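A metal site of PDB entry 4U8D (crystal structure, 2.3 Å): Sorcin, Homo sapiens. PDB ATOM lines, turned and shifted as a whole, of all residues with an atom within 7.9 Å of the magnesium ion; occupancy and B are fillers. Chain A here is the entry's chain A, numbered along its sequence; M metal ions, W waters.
Water W1 bridges the side-chain amide oxygen (OE1) of Gln 48 and the side-chain carboxylate (OD2) of Asp 85.
The backbone NH (N) of Gly 88 lies within hydrogen-bond range of the side-chain carboxylate (OD2) of Asp 83, 2.8 Å away. N of Met 86 lies close to OD1 of Asp 83, at 3.4 Å.
The nearest printed residue that does not touch the magnesium ion is Met 90 (4.3 Å).
The side-chain hydroxyl (OG) of Ser 87 binds the magnesium ion (2.1 Å). The magnesium ion is bound by O of Thr 89 (2.2 Å). The magnesium ion is bound by OD1 of Asp 85. OD1 of Asp 83 binds the magnesium ion (2.2 Å). The magnesium ion is bound by water W2 (2.5 Å). The magnesium ion has five donor atoms within binding distance. Slightly farther from the magnesium ion lies water W1 (2.7 Å).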
ATOM      1  N   GLN A  48     -12.996  14.298  -3.520  1.00  0.00           N
ATOM      2  CA  GLN A  48     -12.817  15.728  -3.795  1.00  0.00           C
ATOM      3  C   GLN A  48     -11.875  16.407  -2.801  1.00  0.00           C
ATOM      4  O   GLN A  48     -11.849  16.054  -1.621  1.00  0.00           O
ATOM      5  CB  GLN A  48     -14.177  16.440  -3.738  1.00  0.00           C
ATOM      6  CG  GLN A  48     -15.142  15.977  -4.845  1.00  0.00           C
ATOM      7  CD  GLN A  48     -14.841  16.640  -6.179  1.00  0.00           C
ATOM      8  OE1 GLN A  48     -14.712  17.873  -6.248  1.00  0.00           O
ATOM      9  NE2 GLN A  48     -14.723  15.845  -7.226  1.00  0.00           N
ATOM     10  N   ILE A  49     -11.109  17.377  -3.289  1.00  0.00           N
ATOM     11  CA  ILE A  49     -10.235  18.196  -2.457  1.00  0.00           C
ATOM     12  C   ILE A  49     -10.589  19.675  -2.604  1.00  0.00           C
ATOM     13  O   ILE A  49     -11.051  20.098  -3.638  1.00  0.00           O
ATOM     14  CB  ILE A  49      -8.732  18.027  -2.823  1.00  0.00           C
ATOM     15  CG1 ILE A  49      -8.465  18.419  -4.283  1.00  0.00           C
ATOM     16  CG2 ILE A  49      -8.245  16.611  -2.525  1.00  0.00           C
ATOM     17  CD1 ILE A  49      -7.017  18.308  -4.690  1.00  0.00           C
ATOM     18  N   VAL A  79      -7.850  26.081  -7.905  1.00  0.00           N
ATOM     19  CA  VAL A  79      -9.150  25.449  -7.777  1.00  0.00           C
ATOM     20  C   VAL A  79     -10.178  26.106  -8.699  1.00  0.00           C
ATOM     21  O   VAL A  79     -10.843  25.427  -9.495  1.00  0.00           O
ATOM     22  CB  VAL A  79      -9.670  25.449  -6.314  1.00  0.00           C
ATOM     23  CG1 VAL A  79     -11.120  25.006  -6.246  1.00  0.00           C
ATOM     24  CG2 VAL A  79      -8.799  24.524  -5.463  1.00  0.00           C
ATOM     25  N   LEU A  82     -10.046  25.184 -12.378  1.00  0.00           N
ATOM     26  CA  LEU A  82     -10.546  23.877 -12.803  1.00  0.00           C
ATOM     27  C   LEU A  82     -11.952  23.535 -12.303  1.00  0.00           C
ATOM     28  O   LEU A  82     -12.411  22.409 -12.458  1.00  0.00           O
ATOM     29  CB  LEU A  82      -9.537  22.819 -12.409  1.00  0.00           C
ATOM     30  CG  LEU A  82      -8.504  22.513 -13.497  1.00  0.00           C
ATOM     31  CD1 LEU A  82      -8.051  23.756 -14.233  1.00  0.00           C
ATOM     32  CD2 LEU A  82      -7.295  21.876 -12.902  1.00  0.00           C
ATOM     33  N   ASP A  83     -12.623  24.516 -11.694  1.00  0.00           N
ATOM     34  CA  ASP A  83     -13.890  24.247 -11.016  1.00  0.00           C
ATOM     35  C   ASP A  83     -15.089  24.419 -11.942  1.00  0.00           C
ATOM     36  O   ASP A  83     -15.854  25.368 -11.815  1.00  0.00           O
ATOM     37  CB  ASP A  83     -14.036  25.160  -9.802  1.00  0.00           C
ATOM     38  CG  ASP A  83     -15.088  24.690  -8.829  1.00  0.00           C
ATOM     39  OD1 ASP A  83     -15.596  23.513  -8.930  1.00  0.00           O
ATOM     40  OD2 ASP A  83     -15.360  25.502  -7.938  1.00  0.00           O
ATOM     41  N   ARG A  84     -15.275  23.455 -12.841  1.00  0.00           N
ATOM     42  CA  ARG A  84     -16.285  23.526 -13.896  1.00  0.00           C
ATOM     43  C   ARG A  84     -17.711  23.243 -13.464  1.00  0.00           C
ATOM     44  O   ARG A  84     -18.656  23.516 -14.222  1.00  0.00           O
ATOM     45  CB  ARG A  84     -15.907  22.551 -15.013  1.00  0.00           C
ATOM     46  CG  ARG A  84     -14.541  22.858 -15.589  1.00  0.00           C
ATOM     47  CD  ARG A  84     -14.268  22.092 -16.874  1.00  0.00           C
ATOM     48  NE  ARG A  84     -12.939  22.438 -17.387  1.00  0.00           N
ATOM     49  CZ  ARG A  84     -11.799  21.777 -17.109  1.00  0.00           C
ATOM     50  NH1 ARG A  84     -10.664  22.205 -17.662  1.00  0.00           N
ATOM     51  NH2 ARG A  84     -11.776  20.678 -16.340  1.00  0.00           N
ATOM     52  N   ASP A  85     -17.860  22.670 -12.269  1.00  0.00           N
ATOM     53  CA  ASP A  85     -19.179  22.385 -11.664  1.00  0.00           C
ATOM     54  C   ASP A  85     -19.461  23.330 -10.507  1.00  0.00           C
ATOM     55  O   ASP A  85     -20.429  23.144  -9.779  1.00  0.00           O
ATOM     56  CB  ASP A  85     -19.300  20.917 -11.215  1.00  0.00           C
ATOM     57  CG  ASP A  85     -18.228  20.480 -10.187  1.00  0.00           C
ATOM     58  OD1 ASP A  85     -17.318  21.257  -9.826  1.00  0.00           O
ATOM     59  OD2 ASP A  85     -18.301  19.308  -9.750  1.00  0.00           O
ATOM     60  N   MET A  86     -18.626  24.341 -10.337  1.00  0.00           N
ATOM     61  CA  MET A  86     -18.790  25.323  -9.286  1.00  0.00           C
ATOM     62  C   MET A  86     -18.977  24.709  -7.901  1.00  0.00           C
ATOM     63  O   MET A  86     -19.774  25.185  -7.117  1.00  0.00           O
ATOM     64  CB  MET A  86     -19.943  26.255  -9.663  1.00  0.00           C
ATOM     65  CG  MET A  86     -19.678  27.040 -10.960  1.00  0.00           C
ATOM     66  SD  MET A  86     -21.146  27.363 -11.977  1.00  0.00           S
ATOM     67  CE  MET A  86     -20.790  29.004 -12.666  1.00  0.00           C
ATOM     68  N   SER A  87     -18.187  23.662  -7.589  1.00  0.00           N
ATOM     69  CA  SER A  87     -18.248  22.951  -6.303  1.00  0.00           C
ATOM     70  C   SER A  87     -17.344  23.500  -5.206  1.00  0.00           C
ATOM     71  O   SER A  87     -17.478  23.110  -4.074  1.00  0.00           O
ATOM     72  CB  SER A  87     -17.902  21.482  -6.517  1.00  0.00           C
ATOM     73  OG  SER A  87     -16.532  21.292  -6.910  1.00  0.00           O
ATOM     74  N   GLY A  88     -16.411  24.398  -5.550  1.00  0.00           N
ATOM     75  CA  GLY A  88     -15.339  24.802  -4.634  1.00  0.00           C
ATOM     76  C   GLY A  88     -14.290  23.715  -4.398  1.00  0.00           C
ATOM     77  O   GLY A  88     -13.436  23.839  -3.484  1.00  0.00           O
ATOM     78  N   THR A  89     -14.329  22.653  -5.208  1.00  0.00           N
ATOM     79  CA  THR A  89     -13.422  21.517  -5.061  1.00  0.00           C
ATOM     80  C   THR A  89     -13.007  20.980  -6.414  1.00  0.00           C
ATOM     81  O   THR A  89     -13.608  21.358  -7.436  1.00  0.00           O
ATOM     82  CB  THR A  89     -14.072  20.311  -4.314  1.00  0.00           C
ATOM     83  OG1 THR A  89     -15.210  19.819  -5.042  1.00  0.00           O
ATOM     84  CG2 THR A  89     -14.506  20.655  -2.891  1.00  0.00           C
ATOM     85  N   MET A  90     -12.021  20.070  -6.431  1.00  0.00           N
ATOM     86  CA  MET A  90     -11.721  19.322  -7.631  1.00  0.00           C
ATOM     87  C   MET A  90     -11.603  17.835  -7.384  1.00  0.00           C
ATOM     88  O   MET A  90     -11.371  17.413  -6.272  1.00  0.00           O
ATOM     89  CB  MET A  90     -10.488  19.877  -8.390  1.00  0.00           C
ATOM     90  CG  MET A  90      -9.118  19.529  -7.849  1.00  0.00           C
ATOM     91  SD  MET A  90      -7.774  20.297  -8.819  1.00  0.00           S
ATOM     92  CE  MET A  90      -7.892  21.999  -8.302  1.00  0.00           C
ATOM     93  N   GLY A  91     -11.774  17.068  -8.448  1.00  0.00           N
ATOM     94  CA  GLY A  91     -11.555  15.650  -8.442  1.00  0.00           C
ATOM     95  C   GLY A  91     -10.209  15.277  -9.003  1.00  0.00           C
ATOM     96  O   GLY A  91      -9.432  16.130  -9.451  1.00  0.00           O
ATOM     97  N   GLU A  94      -9.235  16.388 -12.659  1.00  0.00           N
ATOM     98  CA  GLU A  94      -8.853  17.786 -12.671  1.00  0.00           C
ATOM     99  C   GLU A  94      -7.468  17.976 -12.053  1.00  0.00           C
ATOM    100  O   GLU A  94      -6.649  18.713 -12.574  1.00  0.00           O
ATOM    101  CB  GLU A  94      -9.909  18.623 -11.974  1.00  0.00           C
ATOM    102  CG  GLU A  94     -11.218  18.733 -12.776  1.00  0.00           C
ATOM    103  CD  GLU A  94     -12.114  17.513 -12.631  1.00  0.00           C
ATOM    104  OE1 GLU A  94     -12.417  17.136 -11.492  1.00  0.00           O
ATOM    105  OE2 GLU A  94     -12.534  16.923 -13.682  1.00  0.00           O
HETATM  106 MG    MG M   1     -15.418  21.318  -8.694  1.00  0.00          MG
HETATM  107  O   HOH W   1     -15.339  18.641  -8.751  1.00  0.00           O
HETATM  108  O   HOH W   2     -13.944  20.910 -10.725  1.00  0.00           O
